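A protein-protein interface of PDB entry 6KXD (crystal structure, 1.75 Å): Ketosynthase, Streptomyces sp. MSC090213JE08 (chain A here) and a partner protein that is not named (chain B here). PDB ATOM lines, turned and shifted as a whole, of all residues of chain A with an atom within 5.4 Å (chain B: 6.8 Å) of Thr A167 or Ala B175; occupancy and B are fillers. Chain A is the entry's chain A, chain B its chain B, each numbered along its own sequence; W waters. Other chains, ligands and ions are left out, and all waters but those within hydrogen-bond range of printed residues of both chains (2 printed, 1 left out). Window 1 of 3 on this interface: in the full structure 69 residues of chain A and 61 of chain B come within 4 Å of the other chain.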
ATOM      1  N   GLY A 110     -24.748   0.675 -17.044  1.00  0.00           N
ATOM      2  CA  GLY A 110     -23.676   0.865 -16.104  1.00  0.00           C
ATOM      3  C   GLY A 110     -22.451   0.097 -16.534  1.00  0.00           C
ATOM      4  O   GLY A 110     -22.566  -0.946 -17.149  1.00  0.00           O
ATOM      5  N   THR A 111     -21.266   0.578 -16.168  1.00  0.00           N
ATOM      6  CA  THR A 111     -20.056  -0.168 -16.396  1.00  0.00           C
ATOM      7  C   THR A 111     -18.965   0.247 -15.417  1.00  0.00           C
ATOM      8  O   THR A 111     -18.938   1.393 -14.964  1.00  0.00           O
ATOM      9  CB  THR A 111     -19.527  -0.005 -17.825  1.00  0.00           C
ATOM     10  OG1 THR A 111     -18.673  -1.129 -18.025  1.00  0.00           O
ATOM     11  CG2 THR A 111     -18.731   1.246 -18.065  1.00  0.00           C
ATOM     12  N   ALA A 145     -16.761   4.469 -22.973  1.00  0.00           N
ATOM     13  CA  ALA A 145     -17.815   3.820 -22.269  1.00  0.00           C
ATOM     14  C   ALA A 145     -19.204   4.242 -22.780  1.00  0.00           C
ATOM     15  O   ALA A 145     -20.132   3.469 -22.663  1.00  0.00           O
ATOM     16  CB  ALA A 145     -17.683   4.120 -20.781  1.00  0.00           C
ATOM     17  N   GLY A 146     -19.310   5.435 -23.354  1.00  0.00           N
ATOM     18  CA  GLY A 146     -20.567   5.977 -23.838  1.00  0.00           C
ATOM     19  C   GLY A 146     -21.163   5.055 -24.867  1.00  0.00           C
ATOM     20  O   GLY A 146     -22.371   4.942 -25.017  1.00  0.00           O
ATOM     21  N   THR A 164     -27.128   6.918 -21.932  1.00  0.00           N
ATOM     22  CA  THR A 164     -26.258   7.355 -20.913  1.00  0.00           C
ATOM     23  C   THR A 164     -25.569   6.133 -20.319  1.00  0.00           C
ATOM     24  O   THR A 164     -26.212   5.247 -19.731  1.00  0.00           O
ATOM     25  CB  THR A 164     -27.028   8.073 -19.798  1.00  0.00           C
ATOM     26  OG1 THR A 164     -27.728   9.162 -20.388  1.00  0.00           O
ATOM     27  CG2 THR A 164     -26.098   8.627 -18.749  1.00  0.00           C
ATOM     28  N   THR A 165     -24.258   6.099 -20.415  1.00  0.00           N
ATOM     29  CA  THR A 165     -23.551   5.078 -19.674  1.00  0.00           C
ATOM     30  C   THR A 165     -23.154   5.641 -18.312  1.00  0.00           C
ATOM     31  O   THR A 165     -22.516   6.666 -18.256  1.00  0.00           O
ATOM     32  CB  THR A 165     -22.271   4.665 -20.387  1.00  0.00           C
ATOM     33  OG1 THR A 165     -22.742   4.165 -21.638  1.00  0.00           O
ATOM     34  CG2 THR A 165     -21.512   3.574 -19.669  1.00  0.00           C
ATOM     35  N   VAL A 166     -23.571   4.947 -17.261  1.00  0.00           N
ATOM     36  CA  VAL A 166     -23.257   5.342 -15.921  1.00  0.00           C
ATOM     37  C   VAL A 166     -21.996   4.574 -15.485  1.00  0.00           C
ATOM     38  O   VAL A 166     -21.945   3.346 -15.452  1.00  0.00           O
ATOM     39  CB  VAL A 166     -24.458   5.138 -14.998  1.00  0.00           C
ATOM     40  CG1 VAL A 166     -24.078   5.496 -13.577  1.00  0.00           C
ATOM     41  CG2 VAL A 166     -25.647   5.988 -15.479  1.00  0.00           C
ATOM     42  N   THR A 167     -20.972   5.312 -15.105  1.00  0.00           N
ATOM     43  CA  THR A 167     -19.671   4.711 -14.806  1.00  0.00           C
ATOM     44  C   THR A 167     -19.426   4.816 -13.294  1.00  0.00           C
ATOM     45  O   THR A 167     -18.487   5.427 -12.899  1.00  0.00           O
ATOM     46  CB  THR A 167     -18.556   5.369 -15.606  1.00  0.00           C
ATOM     47  OG1 THR A 167     -18.465   6.755 -15.284  1.00  0.00           O
ATOM     48  CG2 THR A 167     -18.781   5.204 -17.105  1.00  0.00           C
ATOM     49  N   THR A 168     -20.342   4.256 -12.517  1.00  0.00           N
ATOM     50  CA  THR A 168     -20.223   4.222 -11.063  1.00  0.00           C
ATOM     51  C   THR A 168     -19.888   2.787 -10.631  1.00  0.00           C
ATOM     52  O   THR A 168     -20.366   2.264  -9.576  1.00  0.00           O
ATOM     53  CB  THR A 168     -21.481   4.799 -10.414  1.00  0.00           C
ATOM     54  OG1 THR A 168     -22.604   4.016 -10.816  1.00  0.00           O
ATOM     55  CG2 THR A 168     -21.724   6.251 -10.755  1.00  0.00           C
ATOM     56  N   ALA A 169     -19.155   2.103 -11.507  1.00  0.00           N
ATOM     57  CA  ALA A 169     -18.553   0.791 -11.206  1.00  0.00           C
ATOM     58  C   ALA A 169     -19.581  -0.224 -10.673  1.00  0.00           C
ATOM     59  O   ALA A 169     -20.591  -0.527 -11.333  1.00  0.00           O
ATOM     60  CB  ALA A 169     -17.365   1.024 -10.328  1.00  0.00           C
ATOM     61  N   ALA A 172     -23.213   0.609 -10.686  1.00  0.00           N
ATOM     62  CA  ALA A 172     -23.669   1.303 -11.878  1.00  0.00           C
ATOM     63  C   ALA A 172     -25.020   0.735 -12.328  1.00  0.00           C
ATOM     64  O   ALA A 172     -25.888   1.475 -12.722  1.00  0.00           O
ATOM     65  CB  ALA A 172     -22.595   1.237 -12.928  1.00  0.00           C
ATOM     66  N   LEU B 118     -20.650  14.103 -12.925  1.00  0.00           N
ATOM     67  CA  LEU B 118     -19.598  14.467 -13.795  1.00  0.00           C
ATOM     68  C   LEU B 118     -19.654  13.609 -15.063  1.00  0.00           C
ATOM     69  O   LEU B 118     -19.779  12.412 -14.958  1.00  0.00           O
ATOM     70  CB  LEU B 118     -18.262  14.258 -13.107  1.00  0.00           C
ATOM     71  CG  LEU B 118     -17.050  14.841 -13.827  1.00  0.00           C
ATOM     72  CD1 LEU B 118     -17.073  16.369 -13.879  1.00  0.00           C
ATOM     73  CD2 LEU B 118     -15.753  14.378 -13.163  1.00  0.00           C
ATOM     74  N   GLY B 119     -19.595  14.254 -16.223  1.00  0.00           N
ATOM     75  CA  GLY B 119     -19.447  13.528 -17.500  1.00  0.00           C
ATOM     76  C   GLY B 119     -17.974  13.353 -17.889  1.00  0.00           C
ATOM     77  O   GLY B 119     -17.092  14.224 -17.697  1.00  0.00           O
ATOM     78  N   ILE B 120     -17.692  12.195 -18.488  1.00  0.00           N
ATOM     79  CA  ILE B 120     -16.347  11.822 -18.901  1.00  0.00           C
ATOM     80  C   ILE B 120     -16.472  11.145 -20.264  1.00  0.00           C
ATOM     81  O   ILE B 120     -17.581  10.912 -20.709  1.00  0.00           O
ATOM     82  CB  ILE B 120     -15.694  10.856 -17.899  1.00  0.00           C
ATOM     83  CG1 ILE B 120     -16.507   9.571 -17.741  1.00  0.00           C
ATOM     84  CG2 ILE B 120     -15.460  11.565 -16.577  1.00  0.00           C
ATOM     85  CD1 ILE B 120     -15.829   8.448 -16.937  1.00  0.00           C
ATOM     86  N   THR B 121     -15.315  10.861 -20.865  1.00  0.00           N
ATOM     87  CA  THR B 121     -15.207  10.023 -22.066  1.00  0.00           C
ATOM     88  C   THR B 121     -14.875   8.607 -21.600  1.00  0.00           C
ATOM     89  O   THR B 121     -15.663   7.646 -21.711  1.00  0.00           O
ATOM     90  CB  THR B 121     -14.175  10.584 -23.040  1.00  0.00           C
ATOM     91  OG1 THR B 121     -14.494  11.911 -23.438  1.00  0.00           O
ATOM     92  CG2 THR B 121     -14.052   9.741 -24.288  1.00  0.00           C
ATOM     93  N   MET B 122     -13.707   8.481 -20.976  1.00  0.00           N
ATOM     94  CA  MET B 122     -13.297   7.194 -20.510  1.00  0.00           C
ATOM     95  C   MET B 122     -12.315   7.370 -19.371  1.00  0.00           C
ATOM     96  O   MET B 122     -11.425   6.562 -19.174  1.00  0.00           O
ATOM     97  CB  MET B 122     -12.638   6.429 -21.665  1.00  0.00           C
ATOM     98  CG  MET B 122     -12.520   4.954 -21.438  1.00  0.00           C
ATOM     99  SD  MET B 122     -13.988   4.211 -20.793  1.00  0.00           S
ATOM    100  CE  MET B 122     -13.437   2.525 -20.526  1.00  0.00           C
ATOM    101  N   SER B 153     -10.383   4.560 -11.087  1.00  0.00           N
ATOM    102  CA  SER B 153     -11.809   4.318 -11.208  1.00  0.00           C
ATOM    103  C   SER B 153     -12.423   5.425 -12.081  1.00  0.00           C
ATOM    104  O   SER B 153     -12.074   6.581 -11.949  1.00  0.00           O
ATOM    105  CB  SER B 153     -12.420   4.295  -9.856  1.00  0.00           C
ATOM    106  OG  SER B 153     -13.679   3.672  -9.914  1.00  0.00           O
ATOM    107  N   LEU B 154     -13.341   5.075 -12.969  1.00  0.00           N
ATOM    108  CA  LEU B 154     -13.943   6.107 -13.809  1.00  0.00           C
ATOM    109  C   LEU B 154     -14.682   7.159 -12.952  1.00  0.00           C
ATOM    110  O   LEU B 154     -14.789   8.277 -13.381  1.00  0.00           O
ATOM    111  CB  LEU B 154     -14.865   5.460 -14.850  1.00  0.00           C
ATOM    112  CG  LEU B 154     -14.180   4.536 -15.879  1.00  0.00           C
ATOM    113  CD1 LEU B 154     -15.213   3.942 -16.834  1.00  0.00           C
ATOM    114  CD2 LEU B 154     -13.114   5.302 -16.678  1.00  0.00           C
ATOM    115  N   ASN B 155     -15.223   6.761 -11.810  1.00  0.00           N
ATOM    116  CA  ASN B 155     -15.988   7.610 -10.968  1.00  0.00           C
ATOM    117  C   ASN B 155     -15.088   8.322  -9.965  1.00  0.00           C
ATOM    118  O   ASN B 155     -15.587   8.989  -9.079  1.00  0.00           O
ATOM    119  CB  ASN B 155     -17.123   6.861 -10.287  1.00  0.00           C
ATOM    120  CG  ASN B 155     -16.669   5.750  -9.367  1.00  0.00           C
ATOM    121  OD1 ASN B 155     -15.472   5.393  -9.376  1.00  0.00           O
ATOM    122  ND2 ASN B 155     -17.617   5.185  -8.645  1.00  0.00           N
ATOM    123  N   HIS B 156     -13.771   8.189 -10.089  1.00  0.00           N
ATOM    124  CA  HIS B 156     -12.904   8.720  -9.067  1.00  0.00           C
ATOM    125  C   HIS B 156     -12.993  10.250  -8.965  1.00  0.00           C
ATOM    126  O   HIS B 156     -12.998  10.753  -7.843  1.00  0.00           O
ATOM    127  CB  HIS B 156     -11.450   8.363  -9.271  1.00  0.00           C
ATOM    128  CG  HIS B 156     -10.640   8.852  -8.126  1.00  0.00           C
ATOM    129  ND1 HIS B 156      -9.934  10.039  -8.170  1.00  0.00           N
ATOM    130  CD2 HIS B 156     -10.496   8.356  -6.872  1.00  0.00           C
ATOM    131  CE1 HIS B 156      -9.338  10.214  -6.980  1.00  0.00           C
ATOM    132  NE2 HIS B 156      -9.645   9.213  -6.201  1.00  0.00           N
ATOM    133  N   THR B 172     -22.550  10.710  -9.059  1.00  0.00           N
ATOM    134  CA  THR B 172     -22.672   9.962 -10.262  1.00  0.00           C
ATOM    135  C   THR B 172     -21.609  10.435 -11.258  1.00  0.00           C
ATOM    136  O   THR B 172     -21.201  11.583 -11.308  1.00  0.00           O
ATOM    137  CB  THR B 172     -24.068  10.120 -10.862  1.00  0.00           C
ATOM    138  OG1 THR B 172     -25.014   9.817  -9.844  1.00  0.00           O
ATOM    139  CG2 THR B 172     -24.299   9.202 -12.042  1.00  0.00           C
ATOM    140  N   THR B 173     -21.159   9.495 -12.099  1.00  0.00           N
ATOM    141  CA  THR B 173     -20.318   9.787 -13.208  1.00  0.00           C
ATOM    142  C   THR B 173     -20.993   9.167 -14.422  1.00  0.00           C
ATOM    143  O   THR B 173     -21.532   8.036 -14.299  1.00  0.00           O
ATOM    144  CB  THR B 173     -18.905   9.212 -13.046  1.00  0.00           C
ATOM    145  OG1 THR B 173     -18.451   9.729 -11.798  1.00  0.00           O
ATOM    146  CG2 THR B 173     -17.952   9.619 -14.140  1.00  0.00           C
ATOM    147  N   VAL B 174     -21.030   9.921 -15.513  1.00  0.00           N
ATOM    148  CA  VAL B 174     -21.666   9.442 -16.726  1.00  0.00           C
ATOM    149  C   VAL B 174     -20.632   9.626 -17.824  1.00  0.00           C
ATOM    150  O   VAL B 174     -19.797  10.473 -17.793  1.00  0.00           O
ATOM    151  CB  VAL B 174     -22.996  10.140 -17.076  1.00  0.00           C
ATOM    152  CG1 VAL B 174     -24.051   9.875 -16.021  1.00  0.00           C
ATOM    153  CG2 VAL B 174     -22.802  11.632 -17.340  1.00  0.00           C
ATOM    154  N   ALA B 175     -20.657   8.722 -18.794  1.00  0.00           N
ATOM    155  CA  ALA B 175     -19.740   8.812 -19.877  1.00  0.00           C
ATOM    156  C   ALA B 175     -20.464   9.519 -21.019  1.00  0.00           C
ATOM    157  O   ALA B 175     -21.440  10.175 -20.790  1.00  0.00           O
ATOM    158  CB  ALA B 175     -19.273   7.428 -20.272  1.00  0.00           C
ATOM    159  N   GLY B 176     -19.994   9.375 -22.259  1.00  0.00           N
ATOM    160  CA  GLY B 176     -20.689  10.009 -23.359  1.00  0.00           C
ATOM    161  C   GLY B 176     -19.808  10.941 -24.140  1.00  0.00           C
ATOM    162  O   GLY B 176     -20.226  11.495 -25.159  1.00  0.00           O
ATOM    163  N   GLY B 177     -18.586  11.191 -23.665  1.00  0.00           N
ATOM    164  CA  GLY B 177     -17.695  12.032 -24.407  1.00  0.00           C
ATOM    165  C   GLY B 177     -18.238  13.443 -24.576  1.00  0.00           C
ATOM    166  O   GLY B 177     -18.626  14.109 -23.611  1.00  0.00           O
ATOM    167  N   VAL B 179     -20.973  14.665 -25.427  1.00  0.00           N
ATOM    168  CA  VAL B 179     -22.340  14.942 -25.010  1.00  0.00           C
ATOM    169  C   VAL B 179     -22.449  14.783 -23.491  1.00  0.00           C
ATOM    170  O   VAL B 179     -23.538  15.009 -22.955  1.00  0.00           O
ATOM    171  CB  VAL B 179     -23.383  14.079 -25.698  1.00  0.00           C
ATOM    172  CG1 VAL B 179     -23.352  14.346 -27.186  1.00  0.00           C
ATOM    173  CG2 VAL B 179     -23.231  12.604 -25.349  1.00  0.00           C
ATOM    174  N   SER B 180     -21.369  14.329 -22.833  1.00  0.00           N
ATOM    175  CA  SER B 180     -21.488  13.846 -21.453  1.00  0.00           C
ATOM    176  C   SER B 180     -21.933  14.991 -20.517  1.00  0.00           C
ATOM    177  O   SER B 180     -22.603  14.728 -19.511  1.00  0.00           O
ATOM    178  CB  SER B 180     -20.196  13.204 -20.927  1.00  0.00           C
ATOM    179  OG  SER B 180     -19.202  14.213 -20.848  1.00  0.00           O
ATOM    180  N   GLY B 181     -21.484  16.213 -20.765  1.00  0.00           N
ATOM    181  CA  GLY B 181     -21.929  17.371 -19.924  1.00  0.00           C
ATOM    182  C   GLY B 181     -23.429  17.572 -19.993  1.00  0.00           C
ATOM    183  O   GLY B 181     -24.072  17.914 -19.004  1.00  0.00           O
ATOM    184  N   LEU B 183     -25.669  15.025 -20.844  1.00  0.00           N
ATOM    185  CA  LEU B 183     -26.229  13.868 -20.191  1.00  0.00           C
ATOM    186  C   LEU B 183     -26.196  14.116 -18.686  1.00  0.00           C
ATOM    187  O   LEU B 183     -27.142  13.800 -17.997  1.00  0.00           O
ATOM    188  CB  LEU B 183     -25.396  12.651 -20.555  1.00  0.00           C
ATOM    189  CG  LEU B 183     -25.425  12.241 -22.026  1.00  0.00           C
ATOM    190  CD1 LEU B 183     -24.555  11.027 -22.199  1.00  0.00           C
ATOM    191  CD2 LEU B 183     -26.841  11.939 -22.494  1.00  0.00           C
ATOM    192  N   ALA B 184     -25.093  14.698 -18.220  1.00  0.00           N
ATOM    193  CA  ALA B 184     -24.959  14.953 -16.802  1.00  0.00           C
ATOM    194  C   ALA B 184     -26.042  15.958 -16.386  1.00  0.00           C
ATOM    195  O   ALA B 184     -26.647  15.833 -15.352  1.00  0.00           O
ATOM    196  CB  ALA B 184     -23.621  15.490 -16.476  1.00  0.00           C
ATOM    197  N   ALA B 330     -14.843  15.268 -23.320  1.00  0.00           N
ATOM    198  CA  ALA B 330     -15.967  15.283 -22.408  1.00  0.00           C
ATOM    199  C   ALA B 330     -16.230  16.693 -21.875  1.00  0.00           C
ATOM    200  O   ALA B 330     -17.343  16.942 -21.396  1.00  0.00           O
ATOM    201  CB  ALA B 330     -15.779  14.304 -21.270  1.00  0.00           C
HETATM  202  O   HOH W   1     -22.940   7.967 -21.763  1.00  0.00           O
HETATM  203  O   HOH W   2     -28.250  11.247 -18.884  1.00  0.00           O
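The backbone NH of Ala A145 is in hydrogen-bond range of the side-chain sulfur of Met B122.
The backbone NH (N) of Ala B175 sits at hydrogen-bond distance from the backbone carbonyl oxygen (O) of Thr A165 (2.8 Å).
N of Thr A167 lies within hydrogen-bond range of O of Thr B173 (2.9 Å).
O of Leu B118 lies within hydrogen-bond range of N of Val B174 (2.8 Å).
The side-chain hydroxyl (OG) of Ser B153 sits at hydrogen-bond distance from the side-chain amide oxygen (OD1) of Asn B155 (2.5 Å).
The side-chain hydroxyl (OG1) of Thr A168 sits close to the backbone NH (N) of Ala A172, at 3.5 Å.
The backbone NH (N) of Thr A111 lies within hydrogen-bond range of the backbone carbonyl oxygen (O) of Val A166 (2.9 Å).
O of Ile B120 sits at hydrogen-bond distance from N of Gly B176, 3.3 Å away.
N of Ile B120 is in hydrogen-bond range of OG of Ser B180, at 3.5 Å.
Among the printed residues, merely in contact across the chains: Ala A145 with Thr B121 (3.6 Å), Ala A145 with Ala B175 (3.7 Å), Gly A146 with Ala B175 (3.7 Å), Gly A146 with Gly B176 (3.8 Å), Thr A164 with Val B174 (3.6 Å), Thr A164 with Leu B183 (3.6 Å), Thr A165 with Val B174 (3.3 Å), Val A166 with Thr B173 (3.6 Å), Thr A167 with Ile B120 (3.5 Å), Thr A167 with Leu B154 (3.8 Å), Thr A167 with Asn B155 (3.3 Å), Thr A167 with Ala B175 (3.9 Å), Thr A168 with Asn B155 (3.7 Å), Thr A168 with Thr B172 (3.9 Å) and Thr A168 with Thr B173 (3.6 Å).
Printed residues of chain B within 4 Å of Gly A146: Ala B175 (3.7 Å) and Gly B176 (3.8 Å).
Of the printed residues of chain B, Thr A167 touches Ile B120, Leu B154, Asn B155, Thr B173 and Ala B175.
Of chain A, only Ala A145, Gly A146, Thr A165 and Thr A167 come within 4 Å of Ala B175.
Printed residues of chain A within 4 Å of Leu B183: Thr A164 (3.6 Å).
The nearest residue of chain A that does not touch Ala B175 is Val A166 (5.0 Å).
Of the 11 printed residues of chain A, 7 touch a printed residue of chain B.
Among the printed residues, 18 pairs touch across the chains.
Among the printed residues, no Asp or Glu carboxylate lies within 4 Å of a Lys or Arg side-chain nitrogen of the other chain.
Water W2 lies within hydrogen-bond range of OG1 of Thr A164 and O of Leu B183.
Water W1 lies within hydrogen-bond range of N of Thr A165 (2.7 Å), O of Ala B175 (2.8 Å) and N of Gly B176 (3.3 Å).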
